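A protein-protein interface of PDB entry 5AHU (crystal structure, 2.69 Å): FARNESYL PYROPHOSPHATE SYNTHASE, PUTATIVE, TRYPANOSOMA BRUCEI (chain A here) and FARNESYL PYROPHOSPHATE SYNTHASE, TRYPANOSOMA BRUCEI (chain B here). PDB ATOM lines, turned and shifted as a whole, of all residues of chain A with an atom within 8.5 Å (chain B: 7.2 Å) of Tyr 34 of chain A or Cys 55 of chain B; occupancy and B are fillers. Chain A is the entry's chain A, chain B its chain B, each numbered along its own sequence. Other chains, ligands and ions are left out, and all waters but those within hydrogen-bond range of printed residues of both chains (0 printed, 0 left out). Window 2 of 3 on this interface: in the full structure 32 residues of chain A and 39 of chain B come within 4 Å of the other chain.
SG of Cys 55 of chain B is in hydrogen-bond range of OH of Tyr 34 of chain A (3.4 Å).
The side-chain carboxylate (OD2) of Asp 59 of chain B lies within hydrogen-bond range of the side-chain hydroxyl (OH) of Tyr 34 of chain A (2.7 Å).
OG1 of Thr 41 of chain A is in hydrogen-bond range of O of Lys 37 of chain A, 2.7 Å away.
NE1 of Trp 45 of chain B is in hydrogen-bond range of OD2 of Asp 59 of chain B (2.7 Å).
The backbone NH (N) of Cys 55 of chain B is in hydrogen-bond range of the side-chain hydroxyl (OG1) of Thr 52 of chain B.
The side-chain sulfur (SG) of Cys 55 of chain B sits at hydrogen-bond distance from the side-chain carboxylate (OD1) of Asp 59 of chain B, at 3.6 Å.
Among the printed residues, pairs that only touch across the chains: Met 38 of chain A with Trp 45 of chain B (3.2 Å), Met 38 of chain A with Asp 59 of chain B (3.7 Å), Thr 41 of chain A with Trp 45 of chain B (3.7 Å), Tyr 34 of chain A with Trp 45 of chain B (3.8 Å), Tyr 34 of chain A with Val 51 of chain B (3.8 Å) and Leu 35 of chain A with Leu 62 of chain B (3.8 Å).
Tyr 34 of chain A touches just these residues of chain B: Trp 45 (3.8 Å), Val 51 (3.8 Å), Cys 55 (3.4 Å) and Asp 59 (2.7 Å).
Cys 55 of chain B touches just one residue of chain A: Tyr 34 (3.4 Å).
No residue of chain A comes within 4 Å of Ala 56 of chain B.
Printed residues of chain B within 4 Å of Leu 35 of chain A: Leu 62.
Of the printed residues of chain B, Thr 41 of chain A touches Trp 45.
Printed residues of chain B within 4 Å of Met 38 of chain A: Trp 45 (3.2 Å) and Asp 59 (3.7 Å).
Of the printed residues of chain A, Val 51 of chain B touches Tyr 34.
Ile 57 of chain B touches none of the printed residues of chain A.
Arg 36 of chain A touches none of the printed residues of chain B.
The nearest residue of chain B that does not touch Tyr 34 of chain A is Asp 50 of chain B (4.5 Å).
Of the 17 printed residues of chain B, 5 touch a printed residue of chain A.
Hydrophobic or aromatic side chains of chain B that line the printed part of chain A: Trp 45, Val 51 and Leu 62.
Hydrophobic or aromatic side chains of chain A that line the printed part of chain B: Tyr 34, Leu 35 and Met 38.
Among the printed residues, 8 pairs touch across the chains.
Among the printed residues, no Asp or Glu carboxylate lies within 4 Å of a Lys or Arg side-chain nitrogen of the other chain.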
ATOM      1  N   GLN A  14     -10.267  15.540 -22.715  1.00  0.00           N
ATOM      2  CA  GLN A  14     -10.640  14.376 -23.491  1.00  0.00           C
ATOM      3  C   GLN A  14      -9.814  14.290 -24.759  1.00  0.00           C
ATOM      4  O   GLN A  14      -9.390  13.209 -25.149  1.00  0.00           O
ATOM      5  CB  GLN A  14     -12.107  14.376 -23.828  1.00  0.00           C
ATOM      6  CG  GLN A  14     -12.473  13.166 -24.649  1.00  0.00           C
ATOM      7  CD  GLN A  14     -13.955  12.961 -24.712  1.00  0.00           C
ATOM      8  OE1 GLN A  14     -14.628  13.679 -25.432  1.00  0.00           O
ATOM      9  NE2 GLN A  14     -14.476  11.984 -23.962  1.00  0.00           N
ATOM     10  N   LEU A  18      -7.127  11.129 -25.453  1.00  0.00           N
ATOM     11  CA  LEU A  18      -7.414  10.247 -26.573  1.00  0.00           C
ATOM     12  C   LEU A  18      -6.387  10.333 -27.677  1.00  0.00           C
ATOM     13  O   LEU A  18      -6.026   9.320 -28.272  1.00  0.00           O
ATOM     14  CB  LEU A  18      -8.785  10.560 -27.121  1.00  0.00           C
ATOM     15  CG  LEU A  18      -9.856  10.235 -26.094  1.00  0.00           C
ATOM     16  CD1 LEU A  18     -11.191  10.551 -26.737  1.00  0.00           C
ATOM     17  CD2 LEU A  18      -9.790   8.786 -25.622  1.00  0.00           C
ATOM     18  N   MET A  27      -2.652   3.265 -30.555  1.00  0.00           N
ATOM     19  CA  MET A  27      -3.995   2.860 -30.257  1.00  0.00           C
ATOM     20  C   MET A  27      -4.790   3.063 -31.542  1.00  0.00           C
ATOM     21  O   MET A  27      -4.778   4.128 -32.130  1.00  0.00           O
ATOM     22  CB  MET A  27      -4.665   3.580 -29.080  1.00  0.00           C
ATOM     23  CG  MET A  27      -5.998   2.940 -28.743  1.00  0.00           C
ATOM     24  SD  MET A  27      -6.778   3.480 -27.240  1.00  0.00           S
ATOM     25  CE  MET A  27      -5.663   2.642 -26.117  1.00  0.00           C
ATOM     26  N   ASP A  28      -5.517   2.038 -31.938  1.00  0.00           N
ATOM     27  CA  ASP A  28      -6.362   2.116 -33.099  1.00  0.00           C
ATOM     28  C   ASP A  28      -7.614   2.950 -32.824  1.00  0.00           C
ATOM     29  O   ASP A  28      -8.043   3.052 -31.687  1.00  0.00           O
ATOM     30  CB  ASP A  28      -6.756   0.709 -33.523  1.00  0.00           C
ATOM     31  CG  ASP A  28      -7.314  -0.098 -32.388  1.00  0.00           C
ATOM     32  OD1 ASP A  28      -6.521  -0.473 -31.496  1.00  0.00           O
ATOM     33  OD2 ASP A  28      -8.537  -0.356 -32.403  1.00  0.00           O
ATOM     34  N   PRO A  29      -8.234   3.516 -33.879  1.00  0.00           N
ATOM     35  CA  PRO A  29      -9.448   4.321 -33.659  1.00  0.00           C
ATOM     36  C   PRO A  29     -10.617   3.550 -33.003  1.00  0.00           C
ATOM     37  O   PRO A  29     -11.464   4.145 -32.330  1.00  0.00           O
ATOM     38  CB  PRO A  29      -9.835   4.756 -35.092  1.00  0.00           C
ATOM     39  CG  PRO A  29      -8.632   4.485 -35.945  1.00  0.00           C
ATOM     40  CD  PRO A  29      -7.980   3.300 -35.325  1.00  0.00           C
ATOM     41  N   ASN A  30     -10.682   2.240 -33.222  1.00  0.00           N
ATOM     42  CA  ASN A  30     -11.716   1.442 -32.575  1.00  0.00           C
ATOM     43  C   ASN A  30     -11.652   1.561 -31.050  1.00  0.00           C
ATOM     44  O   ASN A  30     -12.595   2.027 -30.437  1.00  0.00           O
ATOM     45  CB  ASN A  30     -11.595  -0.021 -32.990  1.00  0.00           C
ATOM     46  CG  ASN A  30     -12.135  -0.278 -34.367  1.00  0.00           C
ATOM     47  OD1 ASN A  30     -13.211   0.210 -34.729  1.00  0.00           O
ATOM     48  ND2 ASN A  30     -11.421  -1.074 -35.129  1.00  0.00           N
ATOM     49  N   ARG A  31     -10.523   1.178 -30.467  1.00  0.00           N
ATOM     50  CA  ARG A  31     -10.336   1.272 -29.024  1.00  0.00           C
ATOM     51  C   ARG A  31     -10.457   2.702 -28.531  1.00  0.00           C
ATOM     52  O   ARG A  31     -11.085   2.958 -27.491  1.00  0.00           O
ATOM     53  CB  ARG A  31      -9.016   0.624 -28.579  1.00  0.00           C
ATOM     54  CG  ARG A  31      -9.125  -0.870 -28.733  1.00  0.00           C
ATOM     55  CD  ARG A  31      -8.009  -1.681 -28.121  1.00  0.00           C
ATOM     56  NE  ARG A  31      -8.346  -3.093 -28.246  1.00  0.00           N
ATOM     57  CZ  ARG A  31      -8.266  -3.778 -29.376  1.00  0.00           C
ATOM     58  NH1 ARG A  31      -7.808  -3.216 -30.493  1.00  0.00           N
ATOM     59  NH2 ARG A  31      -8.628  -5.047 -29.380  1.00  0.00           N
ATOM     60  N   VAL A  32      -9.902   3.630 -29.298  1.00  0.00           N
ATOM     61  CA  VAL A  32     -10.047   5.027 -28.985  1.00  0.00           C
ATOM     62  C   VAL A  32     -11.536   5.395 -28.892  1.00  0.00           C
ATOM     63  O   VAL A  32     -11.922   6.166 -28.015  1.00  0.00           O
ATOM     64  CB  VAL A  32      -9.356   5.902 -30.034  1.00  0.00           C
ATOM     65  CG1 VAL A  32      -9.569   7.372 -29.729  1.00  0.00           C
ATOM     66  CG2 VAL A  32      -7.867   5.606 -30.089  1.00  0.00           C
ATOM     67  N   ARG A  33     -12.392   4.862 -29.769  1.00  0.00           N
ATOM     68  CA  ARG A  33     -13.827   5.218 -29.693  1.00  0.00           C
ATOM     69  C   ARG A  33     -14.462   4.515 -28.501  1.00  0.00           C
ATOM     70  O   ARG A  33     -15.358   5.050 -27.859  1.00  0.00           O
ATOM     71  CB  ARG A  33     -14.604   4.978 -31.019  1.00  0.00           C
ATOM     72  CG  ARG A  33     -15.667   3.893 -30.976  1.00  0.00           C
ATOM     73  CD  ARG A  33     -16.522   3.862 -32.233  1.00  0.00           C
ATOM     74  NE  ARG A  33     -17.083   2.521 -32.438  1.00  0.00           N
ATOM     75  CZ  ARG A  33     -16.457   1.488 -33.036  1.00  0.00           C
ATOM     76  NH1 ARG A  33     -15.214   1.593 -33.525  1.00  0.00           N
ATOM     77  NH2 ARG A  33     -17.090   0.319 -33.154  1.00  0.00           N
ATOM     78  N   TYR A  34     -13.988   3.325 -28.189  1.00  0.00           N
ATOM     79  CA  TYR A  34     -14.488   2.645 -27.009  1.00  0.00           C
ATOM     80  C   TYR A  34     -14.279   3.520 -25.787  1.00  0.00           C
ATOM     81  O   TYR A  34     -15.195   3.679 -24.975  1.00  0.00           O
ATOM     82  CB  TYR A  34     -13.816   1.285 -26.829  1.00  0.00           C
ATOM     83  CG  TYR A  34     -14.173   0.547 -25.543  1.00  0.00           C
ATOM     84  CD1 TYR A  34     -13.455   0.776 -24.367  1.00  0.00           C
ATOM     85  CD2 TYR A  34     -15.193  -0.403 -25.514  1.00  0.00           C
ATOM     86  CE1 TYR A  34     -13.747   0.105 -23.204  1.00  0.00           C
ATOM     87  CE2 TYR A  34     -15.498  -1.088 -24.339  1.00  0.00           C
ATOM     88  CZ  TYR A  34     -14.773  -0.824 -23.187  1.00  0.00           C
ATOM     89  OH  TYR A  34     -15.044  -1.500 -22.010  1.00  0.00           O
ATOM     90  N   LEU A  35     -13.093   4.112 -25.692  1.00  0.00           N
ATOM     91  CA  LEU A  35     -12.688   4.827 -24.492  1.00  0.00           C
ATOM     92  C   LEU A  35     -13.352   6.158 -24.399  1.00  0.00           C
ATOM     93  O   LEU A  35     -13.595   6.653 -23.311  1.00  0.00           O
ATOM     94  CB  LEU A  35     -11.159   4.993 -24.423  1.00  0.00           C
ATOM     95  CG  LEU A  35     -10.316   3.748 -24.056  1.00  0.00           C
ATOM     96  CD1 LEU A  35      -8.840   4.093 -24.099  1.00  0.00           C
ATOM     97  CD2 LEU A  35     -10.668   3.148 -22.704  1.00  0.00           C
ATOM     98  N   ARG A  36     -13.644   6.746 -25.543  1.00  0.00           N
ATOM     99  CA  ARG A  36     -14.450   7.949 -25.551  1.00  0.00           C
ATOM    100  C   ARG A  36     -15.880   7.664 -24.996  1.00  0.00           C
ATOM    101  O   ARG A  36     -16.372   8.428 -24.176  1.00  0.00           O
ATOM    102  CB  ARG A  36     -14.452   8.578 -26.953  1.00  0.00           C
ATOM    103  CG  ARG A  36     -15.509   9.662 -27.169  1.00  0.00           C
ATOM    104  CD  ARG A  36     -15.615   9.956 -28.641  1.00  0.00           C
ATOM    105  NE  ARG A  36     -14.363  10.545 -29.096  1.00  0.00           N
ATOM    106  CZ  ARG A  36     -14.131  11.858 -29.192  1.00  0.00           C
ATOM    107  NH1 ARG A  36     -15.083  12.749 -28.893  1.00  0.00           N
ATOM    108  NH2 ARG A  36     -12.940  12.291 -29.603  1.00  0.00           N
ATOM    109  N   LYS A  37     -16.522   6.567 -25.384  1.00  0.00           N
ATOM    110  CA  LYS A  37     -17.866   6.306 -24.873  1.00  0.00           C
ATOM    111  C   LYS A  37     -17.792   5.983 -23.392  1.00  0.00           C
ATOM    112  O   LYS A  37     -18.602   6.479 -22.613  1.00  0.00           O
ATOM    113  CB  LYS A  37     -18.602   5.192 -25.621  1.00  0.00           C
ATOM    114  CG  LYS A  37     -18.491   5.308 -27.142  1.00  0.00           C
ATOM    115  CD  LYS A  37     -19.828   5.431 -27.901  1.00  0.00           C
ATOM    116  CE  LYS A  37     -20.325   4.099 -28.472  1.00  0.00           C
ATOM    117  NZ  LYS A  37     -21.728   4.167 -28.988  1.00  0.00           N
ATOM    118  N   MET A  38     -16.826   5.159 -23.002  1.00  0.00           N
ATOM    119  CA  MET A  38     -16.564   4.896 -21.590  1.00  0.00           C
ATOM    120  C   MET A  38     -16.343   6.193 -20.804  1.00  0.00           C
ATOM    121  O   MET A  38     -16.972   6.405 -19.772  1.00  0.00           O
ATOM    122  CB  MET A  38     -15.328   3.990 -21.428  1.00  0.00           C
ATOM    123  CG  MET A  38     -15.085   3.405 -20.032  1.00  0.00           C
ATOM    124  SD  MET A  38     -14.190   4.494 -18.886  1.00  0.00           S
ATOM    125  CE  MET A  38     -12.498   4.180 -19.347  1.00  0.00           C
ATOM    126  N   MET A  39     -15.453   7.061 -21.269  1.00  0.00           N
ATOM    127  CA  MET A  39     -15.221   8.320 -20.549  1.00  0.00           C
ATOM    128  C   MET A  39     -16.476   9.206 -20.382  1.00  0.00           C
ATOM    129  O   MET A  39     -16.725   9.721 -19.298  1.00  0.00           O
ATOM    130  CB  MET A  39     -14.110   9.131 -21.211  1.00  0.00           C
ATOM    131  CG  MET A  39     -13.590  10.266 -20.340  1.00  0.00           C
ATOM    132  SD  MET A  39     -12.565  11.379 -21.299  1.00  0.00           S
ATOM    133  CE  MET A  39     -11.343  10.253 -21.964  1.00  0.00           C
ATOM    134  N   ASP A  40     -17.250   9.387 -21.452  1.00  0.00           N
ATOM    135  CA  ASP A  40     -18.487  10.166 -21.374  1.00  0.00           C
ATOM    136  C   ASP A  40     -19.498   9.485 -20.473  1.00  0.00           C
ATOM    137  O   ASP A  40     -20.113  10.167 -19.661  1.00  0.00           O
ATOM    138  CB  ASP A  40     -19.088  10.380 -22.756  1.00  0.00           C
ATOM    139  CG  ASP A  40     -18.182  11.215 -23.664  1.00  0.00           C
ATOM    140  OD1 ASP A  40     -17.349  11.956 -23.098  1.00  0.00           O
ATOM    141  OD2 ASP A  40     -18.302  11.129 -24.923  1.00  0.00           O
ATOM    142  N   THR A  41     -19.631   8.156 -20.579  1.00  0.00           N
ATOM    143  CA  THR A  41     -20.631   7.423 -19.775  1.00  0.00           C
ATOM    144  C   THR A  41     -20.337   7.387 -18.279  1.00  0.00           C
ATOM    145  O   THR A  41     -21.246   7.311 -17.453  1.00  0.00           O
ATOM    146  CB  THR A  41     -20.792   5.960 -20.195  1.00  0.00           C
ATOM    147  OG1 THR A  41     -20.993   5.877 -21.615  1.00  0.00           O
ATOM    148  CG2 THR A  41     -21.992   5.372 -19.482  1.00  0.00           C
ATOM    149  N   VAL B  28     -17.481   3.133 -10.882  1.00  0.00           N
ATOM    150  CA  VAL B  28     -17.337   1.952 -11.727  1.00  0.00           C
ATOM    151  C   VAL B  28     -17.025   0.742 -10.860  1.00  0.00           C
ATOM    152  O   VAL B  28     -17.703  -0.294 -10.929  1.00  0.00           O
ATOM    153  CB  VAL B  28     -16.246   2.157 -12.781  1.00  0.00           C
ATOM    154  CG1 VAL B  28     -15.859   0.854 -13.395  1.00  0.00           C
ATOM    155  CG2 VAL B  28     -16.750   3.086 -13.852  1.00  0.00           C
ATOM    156  N   ILE B  32     -19.681  -2.741  -9.305  1.00  0.00           N
ATOM    157  CA  ILE B  32     -19.251  -4.129  -9.333  1.00  0.00           C
ATOM    158  C   ILE B  32     -19.240  -4.702  -7.904  1.00  0.00           C
ATOM    159  O   ILE B  32     -19.876  -5.690  -7.615  1.00  0.00           O
ATOM    160  CB  ILE B  32     -17.858  -4.240  -9.983  1.00  0.00           C
ATOM    161  CG1 ILE B  32     -17.899  -3.644 -11.384  1.00  0.00           C
ATOM    162  CG2 ILE B  32     -17.403  -5.693 -10.049  1.00  0.00           C
ATOM    163  CD1 ILE B  32     -16.584  -3.648 -12.126  1.00  0.00           C
ATOM    164  N   TRP B  45     -21.761   0.660 -15.783  1.00  0.00           N
ATOM    165  CA  TRP B  45     -20.758   0.380 -16.817  1.00  0.00           C
ATOM    166  C   TRP B  45     -20.475  -1.121 -17.035  1.00  0.00           C
ATOM    167  O   TRP B  45     -20.362  -1.587 -18.193  1.00  0.00           O
ATOM    168  CB  TRP B  45     -19.442   1.087 -16.501  1.00  0.00           C
ATOM    169  CG  TRP B  45     -18.473   0.950 -17.606  1.00  0.00           C
ATOM    170  CD1 TRP B  45     -17.296   0.262 -17.597  1.00  0.00           C
ATOM    171  CD2 TRP B  45     -18.631   1.449 -18.938  1.00  0.00           C
ATOM    172  NE1 TRP B  45     -16.689   0.335 -18.837  1.00  0.00           N
ATOM    173  CE2 TRP B  45     -17.492   1.064 -19.671  1.00  0.00           C
ATOM    174  CE3 TRP B  45     -19.622   2.197 -19.577  1.00  0.00           C
ATOM    175  CZ2 TRP B  45     -17.322   1.394 -21.023  1.00  0.00           C
ATOM    176  CZ3 TRP B  45     -19.438   2.546 -20.920  1.00  0.00           C
ATOM    177  CH2 TRP B  45     -18.298   2.134 -21.627  1.00  0.00           C
ATOM    178  N   TYR B  46     -20.354  -1.873 -15.939  1.00  0.00           N
ATOM    179  CA  TYR B  46     -20.090  -3.315 -16.011  1.00  0.00           C
ATOM    180  C   TYR B  46     -21.309  -4.096 -16.527  1.00  0.00           C
ATOM    181  O   TYR B  46     -21.174  -5.250 -16.900  1.00  0.00           O
ATOM    182  CB  TYR B  46     -19.587  -3.874 -14.652  1.00  0.00           C
ATOM    183  CG  TYR B  46     -20.645  -4.209 -13.617  1.00  0.00           C
ATOM    184  CD1 TYR B  46     -21.247  -3.217 -12.859  1.00  0.00           C
ATOM    185  CD2 TYR B  46     -21.028  -5.528 -13.392  1.00  0.00           C
ATOM    186  CE1 TYR B  46     -22.216  -3.526 -11.913  1.00  0.00           C
ATOM    187  CE2 TYR B  46     -21.983  -5.864 -12.445  1.00  0.00           C
ATOM    188  CZ  TYR B  46     -22.582  -4.864 -11.702  1.00  0.00           C
ATOM    189  OH  TYR B  46     -23.526  -5.187 -10.747  1.00  0.00           O
ATOM    190  N   ASP B  50     -21.996  -4.646 -24.120  1.00  0.00           N
ATOM    191  CA  ASP B  50     -20.686  -4.891 -24.756  1.00  0.00           C
ATOM    192  C   ASP B  50     -19.473  -4.689 -23.871  1.00  0.00           C
ATOM    193  O   ASP B  50     -18.371  -4.507 -24.388  1.00  0.00           O
ATOM    194  CB  ASP B  50     -20.489  -3.922 -25.897  1.00  0.00           C
ATOM    195  N   VAL B  51     -19.688  -4.688 -22.561  1.00  0.00           N
ATOM    196  CA  VAL B  51     -18.646  -4.491 -21.639  1.00  0.00           C
ATOM    197  C   VAL B  51     -18.619  -5.734 -20.780  1.00  0.00           C
ATOM    198  O   VAL B  51     -19.632  -6.197 -20.258  1.00  0.00           O
ATOM    199  CB  VAL B  51     -18.900  -3.246 -20.801  1.00  0.00           C
ATOM    200  CG1 VAL B  51     -17.889  -3.146 -19.683  1.00  0.00           C
ATOM    201  CG2 VAL B  51     -18.816  -1.999 -21.651  1.00  0.00           C
ATOM    202  N   THR B  52     -17.435  -6.283 -20.624  1.00  0.00           N
ATOM    203  CA  THR B  52     -17.291  -7.456 -19.816  1.00  0.00           C
ATOM    204  C   THR B  52     -16.929  -6.973 -18.417  1.00  0.00           C
ATOM    205  O   THR B  52     -16.398  -5.854 -18.254  1.00  0.00           O
ATOM    206  CB  THR B  52     -16.195  -8.338 -20.387  1.00  0.00           C
ATOM    207  OG1 THR B  52     -14.924  -7.808 -19.995  1.00  0.00           O
ATOM    208  CG2 THR B  52     -16.303  -8.372 -21.933  1.00  0.00           C
ATOM    209  N   VAL B  53     -17.213  -7.817 -17.422  1.00  0.00           N
ATOM    210  CA  VAL B  53     -16.897  -7.490 -16.029  1.00  0.00           C
ATOM    211  C   VAL B  53     -15.399  -7.256 -15.886  1.00  0.00           C
ATOM    212  O   VAL B  53     -14.984  -6.277 -15.288  1.00  0.00           O
ATOM    213  CB  VAL B  53     -17.336  -8.597 -15.055  1.00  0.00           C
ATOM    214  CG1 VAL B  53     -17.046  -8.210 -13.620  1.00  0.00           C
ATOM    215  CG2 VAL B  53     -18.828  -8.846 -15.188  1.00  0.00           C
ATOM    216  N   GLN B  54     -14.583  -8.142 -16.447  1.00  0.00           N
ATOM    217  CA  GLN B  54     -13.134  -7.945 -16.367  1.00  0.00           C
ATOM    218  C   GLN B  54     -12.699  -6.636 -17.029  1.00  0.00           C
ATOM    219  O   GLN B  54     -11.933  -5.882 -16.449  1.00  0.00           O
ATOM    220  CB  GLN B  54     -12.325  -9.152 -16.883  1.00  0.00           C
ATOM    221  CG  GLN B  54     -12.560  -9.574 -18.325  1.00  0.00           C
ATOM    222  CD  GLN B  54     -13.782 -10.468 -18.517  1.00  0.00           C
ATOM    223  OE1 GLN B  54     -14.755 -10.439 -17.719  1.00  0.00           O
ATOM    224  NE2 GLN B  54     -13.752 -11.256 -19.601  1.00  0.00           N
ATOM    225  N   CYS B  55     -13.224  -6.317 -18.206  1.00  0.00           N
ATOM    226  CA  CYS B  55     -12.834  -5.056 -18.835  1.00  0.00           C
ATOM    227  C   CYS B  55     -13.334  -3.845 -18.028  1.00  0.00           C
ATOM    228  O   CYS B  55     -12.677  -2.827 -17.996  1.00  0.00           O
ATOM    229  CB  CYS B  55     -13.233  -4.978 -20.318  1.00  0.00           C
ATOM    230  SG  CYS B  55     -12.432  -3.566 -21.170  1.00  0.00           S
ATOM    231  N   ALA B  56     -14.476  -3.953 -17.366  1.00  0.00           N
ATOM    232  CA  ALA B  56     -14.955  -2.841 -16.508  1.00  0.00           C
ATOM    233  C   ALA B  56     -14.005  -2.541 -15.336  1.00  0.00           C
ATOM    234  O   ALA B  56     -13.773  -1.356 -15.039  1.00  0.00           O
ATOM    235  CB  ALA B  56     -16.358  -3.106 -15.978  1.00  0.00           C
ATOM    236  N   ILE B  57     -13.462  -3.597 -14.698  1.00  0.00           N
ATOM    237  CA  ILE B  57     -12.485  -3.441 -13.592  1.00  0.00           C
ATOM    238  C   ILE B  57     -11.295  -2.640 -14.113  1.00  0.00           C
ATOM    239  O   ILE B  57     -10.851  -1.668 -13.477  1.00  0.00           O
ATOM    240  CB  ILE B  57     -12.006  -4.802 -12.987  1.00  0.00           C
ATOM    241  CG1 ILE B  57     -13.150  -5.557 -12.278  1.00  0.00           C
ATOM    242  CG2 ILE B  57     -10.902  -4.604 -11.954  1.00  0.00           C
ATOM    243  CD1 ILE B  57     -12.823  -7.000 -11.928  1.00  0.00           C
ATOM    244  N   ASN B  58     -10.808  -3.021 -15.297  1.00  0.00           N
ATOM    245  CA  ASN B  58      -9.702  -2.324 -15.906  1.00  0.00           C
ATOM    246  C   ASN B  58     -10.026  -0.929 -16.357  1.00  0.00           C
ATOM    247  O   ASN B  58      -9.179  -0.060 -16.281  1.00  0.00           O
ATOM    248  CB  ASN B  58      -9.158  -3.087 -17.096  1.00  0.00           C
ATOM    249  CG  ASN B  58      -7.835  -2.508 -17.572  1.00  0.00           C
ATOM    250  OD1 ASN B  58      -6.908  -2.345 -16.786  1.00  0.00           O
ATOM    251  ND2 ASN B  58      -7.757  -2.165 -18.839  1.00  0.00           N
ATOM    252  N   ASP B  59     -11.238  -0.720 -16.850  1.00  0.00           N
ATOM    253  CA  ASP B  59     -11.692   0.622 -17.236  1.00  0.00           C
ATOM    254  C   ASP B  59     -11.681   1.555 -16.018  1.00  0.00           C
ATOM    255  O   ASP B  59     -11.301   2.724 -16.122  1.00  0.00           O
ATOM    256  CB  ASP B  59     -13.094   0.574 -17.849  1.00  0.00           C
ATOM    257  CG  ASP B  59     -13.133  -0.158 -19.223  1.00  0.00           C
ATOM    258  OD1 ASP B  59     -12.081  -0.252 -19.914  1.00  0.00           O
ATOM    259  OD2 ASP B  59     -14.241  -0.632 -19.611  1.00  0.00           O
ATOM    260  N   GLY B  60     -12.075   1.013 -14.869  1.00  0.00           N
ATOM    261  CA  GLY B  60     -12.043   1.743 -13.633  1.00  0.00           C
ATOM    262  C   GLY B  60     -10.658   2.227 -13.303  1.00  0.00           C
ATOM    263  O   GLY B  60     -10.482   3.299 -12.792  1.00  0.00           O
ATOM    264  N   LEU B  61      -9.651   1.425 -13.598  1.00  0.00           N
ATOM    265  CA  LEU B  61      -8.267   1.822 -13.328  1.00  0.00           C
ATOM    266  C   LEU B  61      -7.763   2.838 -14.307  1.00  0.00           C
ATOM    267  O   LEU B  61      -7.070   3.747 -13.884  1.00  0.00           O
ATOM    268  CB  LEU B  61      -7.348   0.640 -13.389  1.00  0.00           C
ATOM    269  CG  LEU B  61      -7.668  -0.472 -12.435  1.00  0.00           C
ATOM    270  CD1 LEU B  61      -6.587  -1.473 -12.664  1.00  0.00           C
ATOM    271  CD2 LEU B  61      -7.641  -0.074 -10.986  1.00  0.00           C
ATOM    272  N   LEU B  62      -8.074   2.674 -15.604  1.00  0.00           N
ATOM    273  CA  LEU B  62      -7.813   3.744 -16.589  1.00  0.00           C
ATOM    274  C   LEU B  62      -8.260   5.127 -16.082  1.00  0.00           C
ATOM    275  O   LEU B  62      -7.497   6.099 -16.100  1.00  0.00           O
ATOM    276  CB  LEU B  62      -8.442   3.419 -17.963  1.00  0.00           C
ATOM    277  CG  LEU B  62      -7.689   2.293 -18.699  1.00  0.00           C
ATOM    278  CD1 LEU B  62      -8.425   1.740 -19.916  1.00  0.00           C
ATOM    279  CD2 LEU B  62      -6.276   2.707 -19.087  1.00  0.00           C
